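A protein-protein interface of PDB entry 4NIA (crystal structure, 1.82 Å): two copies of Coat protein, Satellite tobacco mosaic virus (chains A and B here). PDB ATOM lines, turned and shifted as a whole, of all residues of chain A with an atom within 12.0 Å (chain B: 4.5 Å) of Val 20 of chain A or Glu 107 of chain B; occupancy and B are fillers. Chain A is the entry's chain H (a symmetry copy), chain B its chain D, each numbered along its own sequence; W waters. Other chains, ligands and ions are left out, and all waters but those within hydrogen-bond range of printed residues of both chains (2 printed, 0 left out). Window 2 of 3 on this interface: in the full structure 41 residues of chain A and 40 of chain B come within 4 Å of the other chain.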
ATOM      1  N   ASN A  16     -12.287   4.122 -29.796  1.00  0.00           N
ATOM      2  CA  ASN A  16     -11.223   3.451 -28.998  1.00  0.00           C
ATOM      3  C   ASN A  16     -11.439   3.622 -27.485  1.00  0.00           C
ATOM      4  O   ASN A  16     -12.386   4.272 -27.032  1.00  0.00           O
ATOM      5  CB  ASN A  16      -9.841   3.983 -29.409  1.00  0.00           C
ATOM      6  CG  ASN A  16      -8.731   2.960 -29.207  1.00  0.00           C
ATOM      7  OD1 ASN A  16      -8.988   1.761 -29.058  1.00  0.00           O
ATOM      8  ND2 ASN A  16      -7.487   3.431 -29.197  1.00  0.00           N
ATOM      9  N   SER A  17     -10.576   2.985 -26.707  1.00  0.00           N
ATOM     10  CA  SER A  17     -10.629   3.101 -25.264  1.00  0.00           C
ATOM     11  C   SER A  17     -10.337   4.545 -24.879  1.00  0.00           C
ATOM     12  O   SER A  17      -9.458   5.193 -25.453  1.00  0.00           O
ATOM     13  CB  SER A  17      -9.630   2.152 -24.609  1.00  0.00           C
ATOM     14  OG  SER A  17      -9.789   2.191 -23.209  1.00  0.00           O
ATOM     15  N   ASN A  18     -11.120   5.055 -23.944  1.00  0.00           N
ATOM     16  CA  ASN A  18     -10.922   6.379 -23.405  1.00  0.00           C
ATOM     17  C   ASN A  18     -10.375   6.356 -21.983  1.00  0.00           C
ATOM     18  O   ASN A  18     -10.217   7.417 -21.376  1.00  0.00           O
ATOM     19  CB  ASN A  18     -12.243   7.150 -23.383  1.00  0.00           C
ATOM     20  CG  ASN A  18     -12.611   7.764 -24.737  1.00  0.00           C
ATOM     21  OD1 ASN A  18     -13.762   8.108 -24.941  1.00  0.00           O
ATOM     22  ND2 ASN A  18     -11.649   7.880 -25.657  1.00  0.00           N
ATOM     23  N   VAL A  19     -10.172   5.166 -21.411  1.00  0.00           N
ATOM     24  CA  VAL A  19      -9.615   5.061 -20.073  1.00  0.00           C
ATOM     25  C   VAL A  19      -8.382   4.147 -20.014  1.00  0.00           C
ATOM     26  O   VAL A  19      -8.140   3.331 -20.907  1.00  0.00           O
ATOM     27  CB  VAL A  19     -10.657   4.542 -19.022  1.00  0.00           C
ATOM     28  CG1 VAL A  19     -11.769   5.561 -18.794  1.00  0.00           C
ATOM     29  CG2 VAL A  19     -11.248   3.220 -19.452  1.00  0.00           C
ATOM     30  N   VAL A  20      -7.656   4.244 -18.910  1.00  0.00           N
ATOM     31  CA  VAL A  20      -6.575   3.306 -18.634  1.00  0.00           C
ATOM     32  C   VAL A  20      -7.150   1.894 -18.514  1.00  0.00           C
ATOM     33  O   VAL A  20      -8.243   1.692 -17.961  1.00  0.00           O
ATOM     34  CB  VAL A  20      -5.842   3.666 -17.354  1.00  0.00           C
ATOM     35  CG1 VAL A  20      -5.045   4.966 -17.523  1.00  0.00           C
ATOM     36  CG2 VAL A  20      -6.815   3.763 -16.162  1.00  0.00           C
ATOM     37  N   THR A  21      -6.421   0.933 -19.063  1.00  0.00           N
ATOM     38  CA  THR A  21      -6.778  -0.486 -18.951  1.00  0.00           C
ATOM     39  C   THR A  21      -5.559  -1.306 -18.543  1.00  0.00           C
ATOM     40  O   THR A  21      -4.428  -0.931 -18.778  1.00  0.00           O
ATOM     41  CB  THR A  21      -7.319  -1.003 -20.276  1.00  0.00           C
ATOM     42  OG1 THR A  21      -6.368  -0.730 -21.296  1.00  0.00           O
ATOM     43  CG2 THR A  21      -8.635  -0.279 -20.637  1.00  0.00           C
ATOM     44  N   MET A  22      -5.816  -2.432 -17.914  1.00  0.00           N
ATOM     45  CA  MET A  22      -4.778  -3.307 -17.414  1.00  0.00           C
ATOM     46  C   MET A  22      -4.098  -4.080 -18.547  1.00  0.00           C
ATOM     47  O   MET A  22      -4.705  -4.371 -19.573  1.00  0.00           O
ATOM     48  CB  MET A  22      -5.381  -4.282 -16.386  1.00  0.00           C
ATOM     49  CG  MET A  22      -4.351  -5.084 -15.581  1.00  0.00           C
ATOM     50  SD  MET A  22      -4.851  -5.400 -13.894  1.00  0.00           S
ATOM     51  CE  MET A  22      -6.507  -6.048 -14.110  1.00  0.00           C
ATOM     52  N   ILE A  23      -2.806  -4.330 -18.360  1.00  0.00           N
ATOM     53  CA  ILE A  23      -1.983  -5.183 -19.194  1.00  0.00           C
ATOM     54  C   ILE A  23      -1.599  -6.353 -18.294  1.00  0.00           C
ATOM     55  O   ILE A  23      -1.078  -6.174 -17.171  1.00  0.00           O
ATOM     56  CB  ILE A  23      -0.634  -4.481 -19.532  1.00  0.00           C
ATOM     57  CG1 ILE A  23      -0.848  -3.348 -20.505  1.00  0.00           C
ATOM     58  CG2 ILE A  23       0.363  -5.464 -20.103  1.00  0.00           C
ATOM     59  CD1 ILE A  23       0.428  -2.581 -20.776  1.00  0.00           C
ATOM     60  N   ARG A  24      -1.819  -7.562 -18.777  1.00  0.00           N
ATOM     61  CA  ARG A  24      -1.536  -8.752 -17.972  1.00  0.00           C
ATOM     62  C   ARG A  24      -0.100  -9.205 -18.211  1.00  0.00           C
ATOM     63  O   ARG A  24       0.144 -10.215 -18.875  1.00  0.00           O
ATOM     64  CB  ARG A  24      -2.553  -9.858 -18.292  1.00  0.00           C
ATOM     65  CG  ARG A  24      -3.958  -9.476 -17.846  1.00  0.00           C
ATOM     66  CD  ARG A  24      -5.013 -10.528 -18.176  1.00  0.00           C
ATOM     67  NE  ARG A  24      -6.236 -10.271 -17.416  1.00  0.00           N
ATOM     68  CZ  ARG A  24      -7.026  -9.217 -17.601  1.00  0.00           C
ATOM     69  NH1 ARG A  24      -6.743  -8.314 -18.534  1.00  0.00           N
ATOM     70  NH2 ARG A  24      -8.108  -9.059 -16.851  1.00  0.00           N
ATOM     71  N   LEU B  96      -0.166  -0.620  -9.134  1.00  0.00           N
ATOM     72  CA  LEU B  96       0.108   0.624  -9.858  1.00  0.00           C
ATOM     73  C   LEU B  96      -1.144   1.464  -9.911  1.00  0.00           C
ATOM     74  O   LEU B  96      -2.194   0.950 -10.306  1.00  0.00           O
ATOM     75  CB  LEU B  96       0.507   0.362 -11.307  1.00  0.00           C
ATOM     76  CG  LEU B  96       1.813  -0.385 -11.514  1.00  0.00           C
ATOM     77  CD1 LEU B  96       2.024  -0.705 -12.992  1.00  0.00           C
ATOM     78  CD2 LEU B  96       2.961   0.399 -10.954  1.00  0.00           C
ATOM     79  N   LYS B  97      -0.998   2.733  -9.552  1.00  0.00           N
ATOM     80  CA  LYS B  97      -2.044   3.734  -9.701  1.00  0.00           C
ATOM     81  C   LYS B  97      -1.601   4.789 -10.704  1.00  0.00           C
ATOM     82  O   LYS B  97      -0.654   5.516 -10.451  1.00  0.00           O
ATOM     83  CB  LYS B  97      -2.364   4.371  -8.363  1.00  0.00           C
ATOM     84  CG  LYS B  97      -3.458   5.402  -8.444  1.00  0.00           C
ATOM     85  CD  LYS B  97      -3.904   5.880  -7.074  1.00  0.00           C
ATOM     86  CE  LYS B  97      -3.236   7.169  -6.690  1.00  0.00           C
ATOM     87  NZ  LYS B  97      -3.771   7.644  -5.392  1.00  0.00           N
ATOM     88  N   PRO B  98      -2.342   4.927 -11.817  1.00  0.00           N
ATOM     89  CA  PRO B  98      -1.991   5.939 -12.795  1.00  0.00           C
ATOM     90  C   PRO B  98      -2.200   7.343 -12.258  1.00  0.00           C
ATOM     91  O   PRO B  98      -3.223   7.619 -11.627  1.00  0.00           O
ATOM     92  CB  PRO B  98      -2.972   5.685 -13.948  1.00  0.00           C
ATOM     93  CG  PRO B  98      -3.325   4.193 -13.787  1.00  0.00           C
ATOM     94  CD  PRO B  98      -3.371   4.002 -12.315  1.00  0.00           C
ATOM     95  N   PHE B 100      -2.099  11.567 -13.544  1.00  0.00           N
ATOM     96  CA  PHE B 100      -2.212  12.463 -14.707  1.00  0.00           C
ATOM     97  C   PHE B 100      -2.334  13.906 -14.236  1.00  0.00           C
ATOM     98  O   PHE B 100      -3.015  14.185 -13.251  1.00  0.00           O
ATOM     99  CB  PHE B 100      -3.451  12.121 -15.547  1.00  0.00           C
ATOM    100  CG  PHE B 100      -3.419  10.740 -16.134  1.00  0.00           C
ATOM    101  CD1 PHE B 100      -4.199   9.730 -15.593  1.00  0.00           C
ATOM    102  CD2 PHE B 100      -2.582  10.440 -17.200  1.00  0.00           C
ATOM    103  CE1 PHE B 100      -4.158   8.450 -16.108  1.00  0.00           C
ATOM    104  CE2 PHE B 100      -2.554   9.151 -17.727  1.00  0.00           C
ATOM    105  CZ  PHE B 100      -3.348   8.166 -17.192  1.00  0.00           C
ATOM    106  N   SER B 105      -5.993   9.104 -11.352  1.00  0.00           N
ATOM    107  CA  SER B 105      -6.911   7.965 -11.302  1.00  0.00           C
ATOM    108  C   SER B 105      -6.924   7.360  -9.910  1.00  0.00           C
ATOM    109  O   SER B 105      -6.042   7.620  -9.104  1.00  0.00           O
ATOM    110  CB  SER B 105      -6.502   6.912 -12.345  1.00  0.00           C
ATOM    111  OG  SER B 105      -6.541   7.469 -13.650  1.00  0.00           O
ATOM    112  N   THR B 106      -7.933   6.544  -9.634  1.00  0.00           N
ATOM    113  CA  THR B 106      -7.948   5.783  -8.405  1.00  0.00           C
ATOM    114  C   THR B 106      -7.930   4.286  -8.642  1.00  0.00           C
ATOM    115  O   THR B 106      -8.158   3.516  -7.714  1.00  0.00           O
ATOM    116  CB  THR B 106      -9.144   6.183  -7.512  1.00  0.00           C
ATOM    117  OG1 THR B 106     -10.302   6.396  -8.331  1.00  0.00           O
ATOM    118  CG2 THR B 106      -8.813   7.434  -6.739  1.00  0.00           C
ATOM    119  N   GLU B 107      -7.668   3.861  -9.880  1.00  0.00           N
ATOM    120  CA  GLU B 107      -7.429   2.437 -10.158  1.00  0.00           C
ATOM    121  C   GLU B 107      -6.191   1.915  -9.453  1.00  0.00           C
ATOM    122  O   GLU B 107      -5.197   2.607  -9.366  1.00  0.00           O
ATOM    123  CB  GLU B 107      -7.292   2.180 -11.647  1.00  0.00           C
ATOM    124  CG  GLU B 107      -8.641   2.170 -12.378  1.00  0.00           C
ATOM    125  CD  GLU B 107      -9.210   3.571 -12.458  1.00  0.00           C
ATOM    126  OE1 GLU B 107     -10.325   3.824 -11.945  1.00  0.00           O
ATOM    127  OE2 GLU B 107      -8.518   4.388 -13.070  1.00  0.00           O
ATOM    128  N   GLU B 108      -6.265   0.713  -8.907  1.00  0.00           N
ATOM    129  CA  GLU B 108      -5.112   0.086  -8.287  1.00  0.00           C
ATOM    130  C   GLU B 108      -4.878  -1.277  -8.930  1.00  0.00           C
ATOM    131  O   GLU B 108      -5.140  -2.346  -8.345  1.00  0.00           O
ATOM    132  CB  GLU B 108      -5.315  -0.044  -6.779  1.00  0.00           C
ATOM    133  CG  GLU B 108      -5.239   1.331  -6.051  1.00  0.00           C
ATOM    134  CD  GLU B 108      -3.808   1.854  -5.806  1.00  0.00           C
ATOM    135  OE1 GLU B 108      -3.650   2.898  -5.121  1.00  0.00           O
ATOM    136  OE2 GLU B 108      -2.832   1.243  -6.259  1.00  0.00           O
ATOM    137  N   PHE B 109      -4.332  -1.218 -10.128  1.00  0.00           N
ATOM    138  CA  PHE B 109      -4.014  -2.436 -10.863  1.00  0.00           C
ATOM    139  C   PHE B 109      -2.986  -3.284 -10.100  1.00  0.00           C
ATOM    140  O   PHE B 109      -1.902  -2.799  -9.742  1.00  0.00           O
ATOM    141  CB  PHE B 109      -3.469  -2.069 -12.233  1.00  0.00           C
ATOM    142  CG  PHE B 109      -4.424  -1.273 -13.069  1.00  0.00           C
ATOM    143  CD1 PHE B 109      -4.090   0.003 -13.461  1.00  0.00           C
ATOM    144  CD2 PHE B 109      -5.605  -1.832 -13.520  1.00  0.00           C
ATOM    145  CE1 PHE B 109      -4.926   0.739 -14.274  1.00  0.00           C
ATOM    146  CE2 PHE B 109      -6.454  -1.091 -14.334  1.00  0.00           C
ATOM    147  CZ  PHE B 109      -6.107   0.211 -14.689  1.00  0.00           C
ATOM    148  N   TYR B 124      -0.268  -1.253 -17.133  1.00  0.00           N
ATOM    149  CA  TYR B 124      -1.437  -0.578 -17.684  1.00  0.00           C
ATOM    150  C   TYR B 124      -1.073   0.185 -18.925  1.00  0.00           C
ATOM    151  O   TYR B 124       0.075   0.613 -19.107  1.00  0.00           O
ATOM    152  CB  TYR B 124      -2.145   0.341 -16.648  1.00  0.00           C
ATOM    153  CG  TYR B 124      -1.405   1.596 -16.221  1.00  0.00           C
ATOM    154  CD1 TYR B 124      -1.537   2.795 -16.917  1.00  0.00           C
ATOM    155  CD2 TYR B 124      -0.547   1.575 -15.132  1.00  0.00           C
ATOM    156  CE1 TYR B 124      -0.795   3.917 -16.572  1.00  0.00           C
ATOM    157  CE2 TYR B 124       0.152   2.692 -14.761  1.00  0.00           C
ATOM    158  CZ  TYR B 124       0.012   3.872 -15.472  1.00  0.00           C
ATOM    159  OH  TYR B 124       0.731   4.965 -15.063  1.00  0.00           O
ATOM    160  N   ARG B 125      -2.085   0.361 -19.766  1.00  0.00           N
ATOM    161  CA  ARG B 125      -1.992   1.172 -20.981  1.00  0.00           C
ATOM    162  C   ARG B 125      -2.691   2.531 -20.846  1.00  0.00           C
ATOM    163  O   ARG B 125      -3.749   2.660 -20.207  1.00  0.00           O
ATOM    164  CB  ARG B 125      -2.632   0.367 -22.113  1.00  0.00           C
ATOM    165  CG  ARG B 125      -2.639   1.074 -23.440  1.00  0.00           C
ATOM    166  CD  ARG B 125      -3.481   0.317 -24.460  1.00  0.00           C
ATOM    167  NE  ARG B 125      -3.564   1.047 -25.720  1.00  0.00           N
ATOM    168  CZ  ARG B 125      -4.544   1.888 -26.054  1.00  0.00           C
ATOM    169  NH1 ARG B 125      -5.564   2.133 -25.222  1.00  0.00           N
ATOM    170  NH2 ARG B 125      -4.508   2.471 -27.246  1.00  0.00           N
ATOM    171  N   PRO B 127      -4.606   5.457 -22.706  1.00  0.00           N
ATOM    172  CA  PRO B 127      -5.338   5.606 -23.953  1.00  0.00           C
ATOM    173  C   PRO B 127      -4.892   6.874 -24.684  1.00  0.00           C
ATOM    174  O   PRO B 127      -4.315   7.778 -24.073  1.00  0.00           O
ATOM    175  CB  PRO B 127      -6.798   5.716 -23.486  1.00  0.00           C
ATOM    176  CG  PRO B 127      -6.711   6.387 -22.196  1.00  0.00           C
ATOM    177  CD  PRO B 127      -5.437   5.824 -21.543  1.00  0.00           C
HETATM  178  O   HOH W   1      -6.346   1.832 -22.545  1.00  0.00           O
HETATM  179  O   HOH W   2      -6.784   4.566 -26.864  1.00  0.00           O
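Of the 9 printed residues of chain A, 8 touch a printed residue of chain B.
Hydrophobic or aromatic side chains of chain B within 4 Å of the printed part of chain A: Phe 100, Phe 109, Tyr 124 and Pro 127.
Among the printed residues, no Asp or Glu carboxylate lies within 4 Å of a Lys or Arg side-chain nitrogen of the other chain.
Val 20 of chain A touches just these residues of chain B: Phe 100 (3.6 Å), Glu 107 (3.6 Å), Phe 109 (3.9 Å), Arg 125 (3.3 Å) and Pro 127 (3.8 Å).
Glu 107 of chain B touches just one residue of chain A: Val 20 (3.6 Å).
No residue of chain A comes within 4 Å of Thr 106 of chain B.
Tyr 124 of chain B touches two residues of chain A.
Printed residues of chain B within 4 Å of Val 19 of chain A: Pro 127.
Of the printed residues of chain A, Arg 125 of chain B touches Asn 16 (3.7 Å), Val 20 (3.3 Å), Thr 21 (2.9 Å) and Ile 23 (3.98 Å).
Of the printed residues of chain B, Met 22 of chain A touches Phe 109 (3.7 Å).
Printed residues of chain A within 4 Å of Pro 127 of chain B: Ser 17, Asn 18, Val 19 and Val 20.
Printed residues of chain A within 4 Å of Phe 109 of chain B: Val 20 and Met 22.
The nearest printed residue of chain B that does not touch Val 20 of chain A is Tyr 124 of chain B (4.2 Å).
The nearest residue of chain A that does not touch Glu 107 of chain B is Val 19 of chain A (6.3 Å).
The nearest printed residue of chain B that does not touch Ser 17 of chain A is Arg 125 of chain B (4.1 Å).
Water W2 lies within hydrogen-bond range of the side-chain amide nitrogen of Asn 16 of chain A, the backbone carbonyl oxygen of Ser 17 of chain A and the guanidinium group of Arg 125 of chain B.
Water W1 lies within hydrogen-bond range of NH1 of Arg 125 of chain B (2.8 Å), OG1 of Thr 21 of chain A (2.9 Å) and O of Val 19 of chain A (2.9 Å).
No position is printed for both chains.
Of the 14 pairs that touch across the chains among the printed residues, none has its exchanged pair printed and touching as well.
O of Phe 109 of chain B lies within hydrogen-bond range of N of Leu 96 of chain B, at 2.9 Å.
The backbone carbonyl oxygen (O) of Val 19 of chain A sits at hydrogen-bond distance from the side-chain hydroxyl (OG) of Ser 17 of chain A.
Among the printed residues, pairs that only touch across the chains: Asn 16 of chain A with Arg 125 of chain B (3.7 Å), Ser 17 of chain A with Pro 127 of chain B (3.3 Å), Asn 18 of chain A with Pro 127 of chain B (3.7 Å), Val 19 of chain A with Pro 127 of chain B (3.5 Å), Val 20 of chain A with Phe 100 of chain B (3.6 Å), Val 20 of chain A with Glu 107 of chain B (3.6 Å), Val 20 of chain A with Phe 109 of chain B (3.9 Å), Val 20 of chain A with Arg 125 of chain B (3.3 Å), Val 20 of chain A with Pro 127 of chain B (3.8 Å), Thr 21 of chain A with Tyr 124 of chain B (3.2 Å), Met 22 of chain A with Phe 109 of chain B (3.7 Å), Ile 23 of chain A with Tyr 124 of chain B (3.6 Å) and Ile 23 of chain A with Arg 125 of chain B (3.98 Å).
N of Arg 125 of chain B is in hydrogen-bond range of O of Thr 21 of chain A, at 2.9 Å.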
